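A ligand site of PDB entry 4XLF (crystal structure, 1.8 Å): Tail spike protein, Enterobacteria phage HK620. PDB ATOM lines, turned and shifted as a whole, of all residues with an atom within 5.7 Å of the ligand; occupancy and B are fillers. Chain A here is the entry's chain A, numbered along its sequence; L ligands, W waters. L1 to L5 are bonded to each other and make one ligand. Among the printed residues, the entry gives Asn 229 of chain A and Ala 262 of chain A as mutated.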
ATOM      1  N   GLY A 101     -29.906 -26.161 -32.827  1.00  0.00           N
ATOM      2  CA  GLY A 101     -28.634 -26.422 -32.155  1.00  0.00           C
ATOM      3  C   GLY A 101     -28.785 -26.612 -30.641  1.00  0.00           C
ATOM      4  O   GLY A 101     -27.839 -27.052 -29.981  1.00  0.00           O
ATOM      5  N   HIS A 102     -29.939 -26.284 -30.083  1.00  0.00           N
ATOM      6  CA  HIS A 102     -30.207 -26.402 -28.676  1.00  0.00           C
ATOM      7  C   HIS A 102     -31.300 -27.420 -28.405  1.00  0.00           C
ATOM      8  O   HIS A 102     -31.867 -27.428 -27.329  1.00  0.00           O
ATOM      9  CB  HIS A 102     -30.639 -25.063 -28.121  1.00  0.00           C
ATOM     10  CG  HIS A 102     -29.720 -23.940 -28.458  1.00  0.00           C
ATOM     11  ND1 HIS A 102     -28.741 -23.513 -27.606  1.00  0.00           N
ATOM     12  CD2 HIS A 102     -29.682 -23.121 -29.512  1.00  0.00           C
ATOM     13  CE1 HIS A 102     -28.144 -22.452 -28.101  1.00  0.00           C
ATOM     14  NE2 HIS A 102     -28.679 -22.206 -29.290  1.00  0.00           N
ATOM     15  N   SER A 103     -31.527 -28.323 -29.367  1.00  0.00           N
ATOM     16  CA  SER A 103     -32.659 -29.320 -29.235  1.00  0.00           C
ATOM     17  C   SER A 103     -33.951 -28.609 -28.882  1.00  0.00           C
ATOM     18  O   SER A 103     -34.779 -29.164 -28.192  1.00  0.00           O
ATOM     19  CB  SER A 103     -32.352 -30.373 -28.208  1.00  0.00           C
ATOM     20  OG  SER A 103     -31.043 -30.884 -28.417  1.00  0.00           O
ATOM     21  N   GLN A 132     -35.140 -28.824 -25.303  1.00  0.00           N
ATOM     22  CA  GLN A 132     -35.239 -27.593 -24.516  1.00  0.00           C
ATOM     23  C   GLN A 132     -36.455 -26.934 -24.961  1.00  0.00           C
ATOM     24  O   GLN A 132     -36.586 -26.536 -26.142  1.00  0.00           O
ATOM     25  CB  GLN A 132     -34.041 -26.710 -24.740  1.00  0.00           C
ATOM     26  CG  GLN A 132     -32.758 -27.351 -24.192  1.00  0.00           C
ATOM     27  CD  GLN A 132     -31.604 -26.352 -24.087  1.00  0.00           C
ATOM     28  OE1 GLN A 132     -31.662 -25.324 -23.360  1.00  0.00           O
ATOM     29  NE2 GLN A 132     -30.500 -26.698 -24.710  1.00  0.00           N
ATOM     30  N   PHE A 137     -32.423 -18.204 -27.589  1.00  0.00           N
ATOM     31  CA  PHE A 137     -31.351 -18.030 -28.559  1.00  0.00           C
ATOM     32  C   PHE A 137     -31.956 -18.003 -29.979  1.00  0.00           C
ATOM     33  O   PHE A 137     -32.953 -18.657 -30.234  1.00  0.00           O
ATOM     34  CB  PHE A 137     -30.339 -19.176 -28.454  1.00  0.00           C
ATOM     35  CG  PHE A 137     -29.558 -19.241 -27.141  1.00  0.00           C
ATOM     36  CD1 PHE A 137     -28.582 -18.287 -26.838  1.00  0.00           C
ATOM     37  CD2 PHE A 137     -29.741 -20.294 -26.305  1.00  0.00           C
ATOM     38  CE1 PHE A 137     -27.856 -18.421 -25.640  1.00  0.00           C
ATOM     39  CE2 PHE A 137     -29.019 -20.479 -25.160  1.00  0.00           C
ATOM     40  CZ  PHE A 137     -28.053 -19.530 -24.835  1.00  0.00           C
ATOM     41  N   PRO A 142     -24.405 -19.914 -29.341  1.00  0.00           N
ATOM     42  CA  PRO A 142     -24.831 -18.817 -28.467  1.00  0.00           C
ATOM     43  C   PRO A 142     -23.989 -17.563 -28.620  1.00  0.00           C
ATOM     44  O   PRO A 142     -24.505 -16.417 -28.485  1.00  0.00           O
ATOM     45  CB  PRO A 142     -24.748 -19.411 -27.052  1.00  0.00           C
ATOM     46  CG  PRO A 142     -24.041 -20.699 -27.151  1.00  0.00           C
ATOM     47  CD  PRO A 142     -24.118 -21.150 -28.601  1.00  0.00           C
ATOM     48  N   LEU A 172     -28.880 -33.242 -22.787  1.00  0.00           N
ATOM     49  CA  LEU A 172     -29.361 -32.071 -21.981  1.00  0.00           C
ATOM     50  C   LEU A 172     -30.875 -31.879 -22.196  1.00  0.00           C
ATOM     51  O   LEU A 172     -31.433 -32.076 -23.307  1.00  0.00           O
ATOM     52  CB  LEU A 172     -28.613 -30.756 -22.329  1.00  0.00           C
ATOM     53  CG  LEU A 172     -27.073 -30.790 -22.263  1.00  0.00           C
ATOM     54  CD1 LEU A 172     -26.414 -29.641 -23.038  1.00  0.00           C
ATOM     55  CD2 LEU A 172     -26.595 -30.850 -20.852  1.00  0.00           C
ATOM     56  N   ASN A 174     -34.074 -29.065 -20.794  1.00  0.00           N
ATOM     57  CA  ASN A 174     -34.377 -27.756 -20.168  1.00  0.00           C
ATOM     58  C   ASN A 174     -35.856 -27.469 -20.437  1.00  0.00           C
ATOM     59  O   ASN A 174     -36.399 -27.921 -21.440  1.00  0.00           O
ATOM     60  CB  ASN A 174     -33.476 -26.665 -20.774  1.00  0.00           C
ATOM     61  CG  ASN A 174     -33.418 -25.354 -19.961  1.00  0.00           C
ATOM     62  OD1 ASN A 174     -33.959 -25.186 -18.845  1.00  0.00           O
ATOM     63  ND2 ASN A 174     -32.650 -24.407 -20.509  1.00  0.00           N
ATOM     64  N   THR A 197     -32.185 -31.546 -16.984  1.00  0.00           N
ATOM     65  CA  THR A 197     -30.960 -31.062 -16.500  1.00  0.00           C
ATOM     66  C   THR A 197     -31.240 -29.751 -15.679  1.00  0.00           C
ATOM     67  O   THR A 197     -30.693 -29.524 -14.584  1.00  0.00           O
ATOM     68  CB  THR A 197     -30.040 -30.695 -17.659  1.00  0.00           C
ATOM     69  OG1 THR A 197     -29.864 -31.807 -18.564  1.00  0.00           O
ATOM     70  CG2 THR A 197     -28.728 -30.209 -17.090  1.00  0.00           C
ATOM     71  N   TRP A 198     -32.060 -28.915 -16.256  1.00  0.00           N
ATOM     72  CA  TRP A 198     -32.537 -27.620 -15.650  1.00  0.00           C
ATOM     73  C   TRP A 198     -34.035 -27.475 -15.989  1.00  0.00           C
ATOM     74  O   TRP A 198     -34.511 -28.054 -17.019  1.00  0.00           O
ATOM     75  CB  TRP A 198     -31.839 -26.413 -16.241  1.00  0.00           C
ATOM     76  CG  TRP A 198     -30.395 -26.480 -16.414  1.00  0.00           C
ATOM     77  CD1 TRP A 198     -29.452 -26.332 -15.464  1.00  0.00           C
ATOM     78  CD2 TRP A 198     -29.706 -26.713 -17.666  1.00  0.00           C
ATOM     79  NE1 TRP A 198     -28.193 -26.420 -16.051  1.00  0.00           N
ATOM     80  CE2 TRP A 198     -28.336 -26.721 -17.379  1.00  0.00           C
ATOM     81  CE3 TRP A 198     -30.139 -26.939 -18.973  1.00  0.00           C
ATOM     82  CZ2 TRP A 198     -27.361 -26.937 -18.390  1.00  0.00           C
ATOM     83  CZ3 TRP A 198     -29.193 -27.202 -19.960  1.00  0.00           C
ATOM     84  CH2 TRP A 198     -27.816 -27.153 -19.649  1.00  0.00           C
ATOM     85  N   THR A 201     -33.176 -21.685 -17.384  1.00  0.00           N
ATOM     86  CA  THR A 201     -31.911 -21.002 -17.342  1.00  0.00           C
ATOM     87  C   THR A 201     -31.995 -19.557 -17.809  1.00  0.00           C
ATOM     88  O   THR A 201     -32.803 -19.239 -18.694  1.00  0.00           O
ATOM     89  CB  THR A 201     -30.868 -21.661 -18.250  1.00  0.00           C
ATOM     90  OG1 THR A 201     -31.249 -21.538 -19.624  1.00  0.00           O
ATOM     91  CG2 THR A 201     -30.688 -23.108 -17.856  1.00  0.00           C
ATOM     92  N   LEU A 202     -31.241 -18.711 -17.137  1.00  0.00           N
ATOM     93  CA  LEU A 202     -31.325 -17.296 -17.336  1.00  0.00           C
ATOM     94  C   LEU A 202     -29.964 -16.865 -17.825  1.00  0.00           C
ATOM     95  O   LEU A 202     -28.940 -17.178 -17.189  1.00  0.00           O
ATOM     96  CB  LEU A 202     -31.610 -16.563 -16.043  1.00  0.00           C
ATOM     97  CG  LEU A 202     -32.802 -17.029 -15.237  1.00  0.00           C
ATOM     98  CD1 LEU A 202     -32.923 -16.225 -13.940  1.00  0.00           C
ATOM     99  CD2 LEU A 202     -34.088 -17.011 -16.044  1.00  0.00           C
ATOM    100  N   GLY A 203     -29.955 -16.180 -18.928  1.00  0.00           N
ATOM    101  CA  GLY A 203     -28.684 -15.586 -19.409  1.00  0.00           C
ATOM    102  C   GLY A 203     -27.787 -16.590 -20.069  1.00  0.00           C
ATOM    103  O   GLY A 203     -28.081 -17.780 -20.123  1.00  0.00           O
ATOM    104  N   TRP A 204     -26.653 -16.105 -20.552  1.00  0.00           N
ATOM    105  CA  TRP A 204     -25.640 -16.927 -21.199  1.00  0.00           C
ATOM    106  C   TRP A 204     -24.292 -16.316 -20.953  1.00  0.00           C
ATOM    107  O   TRP A 204     -23.985 -15.246 -21.496  1.00  0.00           O
ATOM    108  CB  TRP A 204     -25.874 -17.166 -22.698  1.00  0.00           C
ATOM    109  CG  TRP A 204     -24.784 -17.986 -23.293  1.00  0.00           C
ATOM    110  CD1 TRP A 204     -24.582 -19.312 -23.101  1.00  0.00           C
ATOM    111  CD2 TRP A 204     -23.677 -17.498 -24.049  1.00  0.00           C
ATOM    112  NE1 TRP A 204     -23.419 -19.713 -23.726  1.00  0.00           N
ATOM    113  CE2 TRP A 204     -22.838 -18.624 -24.326  1.00  0.00           C
ATOM    114  CE3 TRP A 204     -23.302 -16.248 -24.536  1.00  0.00           C
ATOM    115  CZ2 TRP A 204     -21.695 -18.514 -25.053  1.00  0.00           C
ATOM    116  CZ3 TRP A 204     -22.160 -16.131 -25.275  1.00  0.00           C
ATOM    117  CH2 TRP A 204     -21.350 -17.269 -25.540  1.00  0.00           C
ATOM    118  N   ASN A 205     -23.496 -17.018 -20.145  1.00  0.00           N
ATOM    119  CA  ASN A 205     -22.116 -16.664 -19.834  1.00  0.00           C
ATOM    120  C   ASN A 205     -21.918 -15.206 -19.557  1.00  0.00           C
ATOM    121  O   ASN A 205     -21.038 -14.581 -20.115  1.00  0.00           O
ATOM    122  CB  ASN A 205     -21.165 -17.149 -20.905  1.00  0.00           C
ATOM    123  CG  ASN A 205     -21.044 -18.644 -20.972  1.00  0.00           C
ATOM    124  OD1 ASN A 205     -21.669 -19.392 -20.194  1.00  0.00           O
ATOM    125  ND2 ASN A 205     -20.300 -19.111 -21.978  1.00  0.00           N
ATOM    126  N   ASN A 229     -26.881 -34.884 -13.818  1.00  0.00           N
ATOM    127  CA  ASN A 229     -26.695 -33.634 -13.057  1.00  0.00           C
ATOM    128  C   ASN A 229     -27.898 -32.808 -13.263  1.00  0.00           C
ATOM    129  O   ASN A 229     -28.473 -32.791 -14.374  1.00  0.00           O
ATOM    130  CB  ASN A 229     -25.456 -32.896 -13.568  1.00  0.00           C
ATOM    131  CG  ASN A 229     -24.857 -31.938 -12.561  1.00  0.00           C
ATOM    132  OD1 ASN A 229     -25.513 -31.424 -11.633  1.00  0.00           O
ATOM    133  ND2 ASN A 229     -23.592 -31.657 -12.770  1.00  0.00           N
ATOM    134  N   HIS A 230     -28.303 -32.127 -12.202  1.00  0.00           N
ATOM    135  CA  HIS A 230     -29.468 -31.273 -12.264  1.00  0.00           C
ATOM    136  C   HIS A 230     -29.342 -30.037 -11.409  1.00  0.00           C
ATOM    137  O   HIS A 230     -28.886 -30.164 -10.279  1.00  0.00           O
ATOM    138  CB  HIS A 230     -30.691 -32.027 -11.796  1.00  0.00           C
ATOM    139  CG  HIS A 230     -31.937 -31.185 -11.746  1.00  0.00           C
ATOM    140  ND1 HIS A 230     -32.909 -31.210 -12.731  1.00  0.00           N
ATOM    141  CD2 HIS A 230     -32.393 -30.339 -10.792  1.00  0.00           C
ATOM    142  CE1 HIS A 230     -33.891 -30.412 -12.383  1.00  0.00           C
ATOM    143  NE2 HIS A 230     -33.606 -29.878 -11.210  1.00  0.00           N
ATOM    144  N   SER A 231     -29.664 -28.894 -11.988  1.00  0.00           N
ATOM    145  CA  SER A 231     -29.806 -27.590 -11.279  1.00  0.00           C
ATOM    146  C   SER A 231     -31.111 -26.946 -11.766  1.00  0.00           C
ATOM    147  O   SER A 231     -31.240 -26.626 -12.926  1.00  0.00           O
ATOM    148  CB  SER A 231     -28.638 -26.648 -11.500  1.00  0.00           C
ATOM    149  OG  SER A 231     -28.816 -25.516 -10.673  1.00  0.00           O
ATOM    150  N   TYR A 234     -30.643 -22.149 -13.333  1.00  0.00           N
ATOM    151  CA  TYR A 234     -29.284 -21.676 -13.481  1.00  0.00           C
ATOM    152  C   TYR A 234     -29.249 -20.183 -13.864  1.00  0.00           C
ATOM    153  O   TYR A 234     -29.816 -19.796 -14.882  1.00  0.00           O
ATOM    154  CB  TYR A 234     -28.584 -22.544 -14.522  1.00  0.00           C
ATOM    155  CG  TYR A 234     -27.069 -22.642 -14.572  1.00  0.00           C
ATOM    156  CD1 TYR A 234     -26.281 -21.596 -15.024  1.00  0.00           C
ATOM    157  CD2 TYR A 234     -26.424 -23.839 -14.274  1.00  0.00           C
ATOM    158  CE1 TYR A 234     -24.879 -21.728 -15.109  1.00  0.00           C
ATOM    159  CE2 TYR A 234     -25.045 -23.949 -14.377  1.00  0.00           C
ATOM    160  CZ  TYR A 234     -24.274 -22.922 -14.815  1.00  0.00           C
ATOM    161  OH  TYR A 234     -22.901 -23.075 -14.982  1.00  0.00           O
ATOM    162  N   ASN A 236     -27.262 -17.214 -15.038  1.00  0.00           N
ATOM    163  CA  ASN A 236     -26.019 -16.935 -15.725  1.00  0.00           C
ATOM    164  C   ASN A 236     -25.999 -15.538 -16.356  1.00  0.00           C
ATOM    165  O   ASN A 236     -25.342 -15.294 -17.339  1.00  0.00           O
ATOM    166  CB  ASN A 236     -25.764 -18.000 -16.780  1.00  0.00           C
ATOM    167  CG  ASN A 236     -24.267 -18.264 -17.011  1.00  0.00           C
ATOM    168  OD1 ASN A 236     -23.430 -17.639 -16.411  1.00  0.00           O
ATOM    169  ND2 ASN A 236     -23.983 -19.180 -17.935  1.00  0.00           N
ATOM    170  N   ALA A 262     -28.357 -22.363  -9.140  1.00  0.00           N
ATOM    171  CA  ALA A 262     -26.981 -21.998  -9.310  1.00  0.00           C
ATOM    172  C   ALA A 262     -26.933 -20.473  -9.514  1.00  0.00           C
ATOM    173  O   ALA A 262     -27.492 -19.973 -10.492  1.00  0.00           O
ATOM    174  CB  ALA A 262     -26.361 -22.679 -10.524  1.00  0.00           C
ATOM    175  N   HIS A 264     -24.487 -17.685 -10.666  1.00  0.00           N
ATOM    176  CA  HIS A 264     -23.201 -17.685 -11.327  1.00  0.00           C
ATOM    177  C   HIS A 264     -22.720 -16.360 -11.918  1.00  0.00           C
ATOM    178  O   HIS A 264     -21.737 -16.352 -12.682  1.00  0.00           O
ATOM    179  CB  HIS A 264     -23.192 -18.759 -12.443  1.00  0.00           C
ATOM    180  CG  HIS A 264     -22.896 -20.158 -11.990  1.00  0.00           C
ATOM    181  ND1 HIS A 264     -22.228 -21.040 -12.800  1.00  0.00           N
ATOM    182  CD2 HIS A 264     -23.169 -20.835 -10.863  1.00  0.00           C
ATOM    183  CE1 HIS A 264     -22.098 -22.209 -12.198  1.00  0.00           C
ATOM    184  NE2 HIS A 264     -22.725 -22.139 -11.050  1.00  0.00           N
ATOM    185  N   TYR A 283     -25.612 -23.508  -5.559  1.00  0.00           N
ATOM    186  CA  TYR A 283     -24.217 -23.155  -5.908  1.00  0.00           C
ATOM    187  C   TYR A 283     -24.070 -21.602  -6.038  1.00  0.00           C
ATOM    188  O   TYR A 283     -24.891 -20.936  -6.637  1.00  0.00           O
ATOM    189  CB  TYR A 283     -23.735 -23.805  -7.225  1.00  0.00           C
ATOM    190  CG  TYR A 283     -23.502 -25.284  -7.096  1.00  0.00           C
ATOM    191  CD1 TYR A 283     -22.262 -25.768  -6.677  1.00  0.00           C
ATOM    192  CD2 TYR A 283     -24.497 -26.222  -7.381  1.00  0.00           C
ATOM    193  CE1 TYR A 283     -22.026 -27.133  -6.558  1.00  0.00           C
ATOM    194  CE2 TYR A 283     -24.247 -27.546  -7.273  1.00  0.00           C
ATOM    195  CZ  TYR A 283     -23.024 -28.008  -6.864  1.00  0.00           C
ATOM    196  OH  TYR A 283     -22.820 -29.363  -6.729  1.00  0.00           O
ATOM    197  N   VAL A 285     -20.977 -19.504  -7.487  1.00  0.00           N
ATOM    198  CA  VAL A 285     -19.725 -19.913  -8.139  1.00  0.00           C
ATOM    199  C   VAL A 285     -19.436 -18.910  -9.221  1.00  0.00           C
ATOM    200  O   VAL A 285     -20.368 -18.464  -9.920  1.00  0.00           O
ATOM    201  CB  VAL A 285     -19.881 -21.325  -8.733  1.00  0.00           C
ATOM    202  CG1 VAL A 285     -18.628 -21.717  -9.587  1.00  0.00           C
ATOM    203  CG2 VAL A 285     -20.090 -22.370  -7.631  1.00  0.00           C
ATOM    204  N   HIS A 287     -17.433 -19.345 -12.517  1.00  0.00           N
ATOM    205  CA  HIS A 287     -16.665 -20.111 -13.505  1.00  0.00           C
ATOM    206  C   HIS A 287     -15.947 -19.148 -14.479  1.00  0.00           C
ATOM    207  O   HIS A 287     -16.608 -18.320 -15.186  1.00  0.00           O
ATOM    208  CB  HIS A 287     -17.569 -20.969 -14.353  1.00  0.00           C
ATOM    209  CG  HIS A 287     -18.092 -22.204 -13.692  1.00  0.00           C
ATOM    210  ND1 HIS A 287     -17.379 -22.989 -12.827  1.00  0.00           N
ATOM    211  CD2 HIS A 287     -19.298 -22.823 -13.823  1.00  0.00           C
ATOM    212  CE1 HIS A 287     -18.104 -24.021 -12.444  1.00  0.00           C
ATOM    213  NE2 HIS A 287     -19.303 -23.912 -12.988  1.00  0.00           N
ATOM    214  N   ALA A 289     -14.896 -19.925 -17.191  1.00  0.00           N
ATOM    215  CA  ALA A 289     -15.512 -20.227 -18.470  1.00  0.00           C
ATOM    216  C   ALA A 289     -16.774 -19.484 -18.816  1.00  0.00           C
ATOM    217  O   ALA A 289     -17.227 -19.549 -19.974  1.00  0.00           O
ATOM    218  CB  ALA A 289     -15.800 -21.738 -18.534  1.00  0.00           C
ATOM    219  N   GLU A 290     -17.407 -18.843 -17.834  1.00  0.00           N
ATOM    220  CA  GLU A 290     -18.633 -18.171 -18.028  1.00  0.00           C
ATOM    221  C   GLU A 290     -18.464 -16.663 -17.884  1.00  0.00           C
ATOM    222  O   GLU A 290     -19.423 -15.963 -17.723  1.00  0.00           O
ATOM    223  CB  GLU A 290     -19.676 -18.708 -16.995  1.00  0.00           C
ATOM    224  CG  GLU A 290     -19.963 -20.186 -17.219  1.00  0.00           C
ATOM    225  CD  GLU A 290     -21.020 -20.732 -16.296  1.00  0.00           C
ATOM    226  OE1 GLU A 290     -21.166 -20.199 -15.166  1.00  0.00           O
ATOM    227  OE2 GLU A 290     -21.689 -21.699 -16.661  1.00  0.00           O
ATOM    228  N   ASN A 361     -14.577 -28.269 -10.904  1.00  0.00           N
ATOM    229  CA  ASN A 361     -15.161 -29.455 -11.520  1.00  0.00           C
ATOM    230  C   ASN A 361     -14.151 -30.560 -11.855  1.00  0.00           C
ATOM    231  O   ASN A 361     -14.544 -31.679 -11.951  1.00  0.00           O
ATOM    232  CB  ASN A 361     -16.010 -29.113 -12.770  1.00  0.00           C
ATOM    233  CG  ASN A 361     -17.308 -28.430 -12.400  1.00  0.00           C
ATOM    234  OD1 ASN A 361     -17.683 -28.423 -11.240  1.00  0.00           O
ATOM    235  ND2 ASN A 361     -17.999 -27.840 -13.376  1.00  0.00           N
HETATM  236  C1  LIG L   1     -23.621 -27.925 -10.942  1.00  0.00           C
HETATM  237  C2  LIG L   1     -23.886 -27.501 -12.391  1.00  0.00           C
HETATM  238  C3  LIG L   1     -22.556 -27.400 -13.153  1.00  0.00           C
HETATM  239  C4  LIG L   1     -21.638 -26.410 -12.378  1.00  0.00           C
HETATM  240  C5  LIG L   1     -21.485 -26.752 -10.851  1.00  0.00           C
HETATM  241  C6  LIG L   1     -20.923 -25.539 -10.040  1.00  0.00           C
HETATM  242  C7  LIG L   1     -25.863 -28.096 -13.713  1.00  0.00           C
HETATM  243  C8  LIG L   1     -26.770 -29.194 -14.126  1.00  0.00           C
HETATM  244  O1  LIG L   1     -22.759 -27.038 -10.271  1.00  0.00           O
HETATM  245  O2  LIG L   1     -22.749 -26.952 -14.504  1.00  0.00           O
HETATM  246  O3  LIG L   1     -20.337 -26.295 -12.952  1.00  0.00           O
HETATM  247  O4  LIG L   1     -22.114 -24.655  -9.849  1.00  0.00           O
HETATM  248  O5  LIG L   1     -26.036 -26.912 -14.101  1.00  0.00           O
HETATM  249  N1  LIG L   1     -24.837 -28.463 -12.920  1.00  0.00           N
HETATM  250  O6  LIG L   1     -23.070 -29.198 -10.941  1.00  0.00           O
HETATM  251  C1  LG2 L   2     -21.797 -27.505 -15.419  1.00  0.00           C
HETATM  252  C2  LG2 L   2     -21.775 -26.509 -16.584  1.00  0.00           C
HETATM  253  C3  LG2 L   2     -23.167 -26.451 -17.281  1.00  0.00           C
HETATM  254  C4  LG2 L   2     -23.655 -27.838 -17.642  1.00  0.00           C
HETATM  255  C5  LG2 L   2     -23.638 -28.721 -16.384  1.00  0.00           C
HETATM  256  C6  LG2 L   2     -24.028 -30.170 -16.608  1.00  0.00           C
HETATM  257  O1  LG2 L   2     -21.436 -25.221 -16.080  1.00  0.00           O
HETATM  258  O2  LG2 L   2     -22.997 -25.646 -18.441  1.00  0.00           O
HETATM  259  O3  LG2 L   2     -22.768 -28.437 -18.634  1.00  0.00           O
HETATM  260  O4  LG2 L   2     -22.301 -28.742 -15.825  1.00  0.00           O
HETATM  261  O5  LG2 L   2     -25.321 -30.253 -17.212  1.00  0.00           O
HETATM  262  C1  LG3 L   3     -23.491 -28.983 -19.750  1.00  0.00           C
HETATM  263  C2  LG3 L   3     -22.514 -29.785 -20.619  1.00  0.00           C
HETATM  264  C3  LG3 L   3     -21.486 -28.863 -21.321  1.00  0.00           C
HETATM  265  C4  LG3 L   3     -22.269 -27.872 -22.139  1.00  0.00           C
HETATM  266  C5  LG3 L   3     -23.195 -27.058 -21.193  1.00  0.00           C
HETATM  267  C6  LG3 L   3     -24.073 -25.999 -21.869  1.00  0.00           C
HETATM  268  O1  LG3 L   3     -21.821 -30.697 -19.784  1.00  0.00           O
HETATM  269  O2  LG3 L   3     -20.727 -29.718 -22.172  1.00  0.00           O
HETATM  270  O3  LG3 L   3     -21.362 -27.023 -22.776  1.00  0.00           O
HETATM  271  O4  LG3 L   3     -24.102 -27.991 -20.547  1.00  0.00           O
HETATM  272  O5  LG3 L   3     -24.838 -26.667 -22.912  1.00  0.00           O
HETATM  273  C1  LG4 L   4     -23.624 -24.349 -18.319  1.00  0.00           C
HETATM  274  C2  LG4 L   4     -22.905 -23.509 -19.393  1.00  0.00           C
HETATM  275  C3  LG4 L   4     -23.569 -22.144 -19.531  1.00  0.00           C
HETATM  276  C4  LG4 L   4     -25.094 -22.167 -19.532  1.00  0.00           C
HETATM  277  C5  LG4 L   4     -25.555 -23.028 -18.422  1.00  0.00           C
HETATM  278  C6  LG4 L   4     -27.022 -23.247 -18.432  1.00  0.00           C
HETATM  279  C7  LG4 L   4     -20.522 -23.875 -19.648  1.00  0.00           C
HETATM  280  C8  LG4 L   4     -19.161 -23.769 -19.035  1.00  0.00           C
HETATM  281  N1  LG4 L   4     -21.536 -23.421 -18.938  1.00  0.00           N
HETATM  282  O1  LG4 L   4     -23.086 -21.571 -20.730  1.00  0.00           O
HETATM  283  O2  LG4 L   4     -25.623 -20.813 -19.360  1.00  0.00           O
HETATM  284  O3  LG4 L   4     -25.021 -24.310 -18.554  1.00  0.00           O
HETATM  285  O4  LG4 L   4     -27.505 -23.828 -19.617  1.00  0.00           O
HETATM  286  O5  LG4 L   4     -20.662 -24.342 -20.785  1.00  0.00           O
HETATM  287  C1  LG5 L   5     -24.428 -26.111 -24.181  1.00  0.00           C
HETATM  288  C2  LG5 L   5     -25.221 -26.863 -25.245  1.00  0.00           C
HETATM  289  C3  LG5 L   5     -26.650 -26.446 -25.242  1.00  0.00           C
HETATM  290  C4  LG5 L   5     -26.790 -24.924 -25.263  1.00  0.00           C
HETATM  291  C5  LG5 L   5     -26.015 -24.353 -24.113  1.00  0.00           C
HETATM  292  C6  LG5 L   5     -25.938 -22.814 -24.181  1.00  0.00           C
HETATM  293  O1  LG5 L   5     -24.633 -26.541 -26.512  1.00  0.00           O
HETATM  294  O2  LG5 L   5     -27.210 -27.008 -26.451  1.00  0.00           O
HETATM  295  O3  LG5 L   5     -28.202 -24.621 -25.228  1.00  0.00           O
HETATM  296  O4  LG5 L   5     -24.629 -24.719 -24.263  1.00  0.00           O
HETATM  297  O   HOH W   1     -18.232 -28.876 -23.284  1.00  0.00           O
HETATM  298  O   HOH W   2     -22.576 -22.552 -23.478  1.00  0.00           O
HETATM  299  O   HOH W   3     -20.374 -29.982 -17.560  1.00  0.00           O
HETATM  300  O   HOH W   4     -26.513 -28.834 -28.159  1.00  0.00           O
HETATM  301  O   HOH W   5     -19.941 -22.005 -22.523  1.00  0.00           O
HETATM  302  O   HOH W   6     -29.079 -29.445 -26.190  1.00  0.00           O
HETATM  303  O   HOH W   7     -23.195 -30.855  -8.896  1.00  0.00           O
HETATM  304  O   HOH W   8     -27.308 -20.175 -21.270  1.00  0.00           O
HETATM  305  O   HOH W   9     -19.425 -31.832 -21.437  1.00  0.00           O
HETATM  306  O   HOH W  10     -28.110 -20.107 -17.527  1.00  0.00           O
HETATM  307  O   HOH W  11     -29.783 -23.438 -23.484  1.00  0.00           O
HETATM  308  O   HOH W  12     -23.213 -32.993 -21.346  1.00  0.00           O
HETATM  309  O   HOH W  13     -21.286 -31.609 -23.843  1.00  0.00           O
HETATM  310  O   HOH W  14     -29.213 -22.329 -21.164  1.00  0.00           O
HETATM  311  O   HOH W  15     -25.953 -32.794 -17.358  1.00  0.00           O
HETATM  312  O   HOH W  16     -18.586 -25.647 -16.003  1.00  0.00           O
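NE2 of His 264 is in hydrogen-bond range of O4 of LIG L1 (2.9 Å).
O3 of LG5 L5 lies within hydrogen-bond range of ND1 of His 102, at 2.7 Å.
ND2 of Asn 361 sits at hydrogen-bond distance from O3 of LIG L1 (2.8 Å).
ND2 of Asn 236 lies within hydrogen-bond range of O2 of LG4 L4 (2.7 Å).
The side-chain carboxylate (OE2) of Glu 290 sits at hydrogen-bond distance from a nitrogen (N1) of LG4 L4, at 2.9 Å.
OH of Tyr 234 sits at hydrogen-bond distance from O1 of LG2 L2, 2.8 Å away.
O1 of LG4 L4 sits at hydrogen-bond distance from OD1 of Asn 205 (2.7 Å).
O6 of LIG L1 lies within hydrogen-bond range of ND2 of Asn 229 (3.1 Å).
The side-chain amide nitrogen of Gln 132 is in hydrogen-bond range of an oxygen (O3) of LG5 L5 (3.1 Å).
A ring nitrogen (NE2) of His 287 lies within hydrogen-bond range of an oxygen (O3) of LIG L1 (2.6 Å).
O5 of LIG L1 is in hydrogen-bond range of NE1 of Trp 198 (2.9 Å).
O of Gly 101 touches O2 of LG5 L5 (3.6 Å).
CZ of Phe 137 touches C6 of LG5 L5 (3.96 Å).
CD1 of Leu 172 touches O5 of LG3 L3, 3.4 Å away.
Thr 197 touches the ligand.
CG2 of Thr 201 touches O4 of LG4 L4, 3.7 Å away.
O of Gly 203 touches O2 of LG4 L4, 3.98 Å away.
Trp 204 touches the ligand.
N of His 230 touches C8 of LIG L1, at 3.8 Å.
N of Ser 231 touches C8 of LIG L1, at 3.6 Å.
CG of Tyr 283 touches O4 of LIG L1, at 3.1 Å.
CG2 of Val 285 touches O4 of LIG L1, 3.8 Å away.
CB of Ala 289 touches C8 of LG4 L4 (3.96 Å).
Hydrophobic or aromatic side chains within 4 Å of the ligand: His 102, Phe 137, Leu 172, Trp 198, Trp 204, Tyr 234, His 264, Tyr 283, Val 285, His 287 and Ala 289.
The nearest printed residue that does not touch the ligand is Pro 142 (4.1 Å).
Water W4 lies within hydrogen-bond range of O2 of LG5 L5 (2.6 Å) and O of Gly 101 (2.9 Å).
Water W7 lies within hydrogen-bond range of an oxygen (O6) of LIG L1 and the side-chain hydroxyl (OH) of Tyr 283.
Water W11 bridges an oxygen (O3) of LG5 L5 (2.6 Å) and the side-chain amide oxygen (OE1) of Gln 132 (2.7 Å).
Water W14 lies within hydrogen-bond range of the side-chain hydroxyl (OG1) of Thr 201 (2.7 Å) and an oxygen (O4) of LG4 L4 (2.7 Å).
Water W5 bridges the side-chain amide nitrogen (ND2) of Asn 205 (3.0 Å) and an oxygen (O5) of LG4 L4 (3.0 Å).
Water W6 lies within hydrogen-bond range of O2 of LG5 L5 (3.1 Å), OG of Ser 103 (3.3 Å) and NE2 of Gln 132 (3.4 Å).
The backbone NH (N) of Leu 202 sits at hydrogen-bond distance from the backbone carbonyl oxygen (O) of Tyr 234 (2.9 Å).
O of Thr 197 lies close to ND1 of His 230, at 3.3 Å.
OH of Tyr 234 lies close to ND1 of His 264 (3.1 Å).
The backbone NH (N) of Gln 132 lies within hydrogen-bond range of the backbone carbonyl oxygen (O) of Ser 103.
N of Asn 205 lies close to ND2 of Asn 236 (3.1 Å).
The side-chain hydroxyl of Thr 201 lies within hydrogen-bond range of the side-chain amide nitrogen of Asn 174, 3.3 Å away.
The backbone carbonyl oxygen (O) of His 102 sits at hydrogen-bond distance from the side-chain amide nitrogen (NE2) of Gln 132 (3.0 Å).
O of Thr 197 lies within hydrogen-bond range of N of Ser 231, 2.9 Å away.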
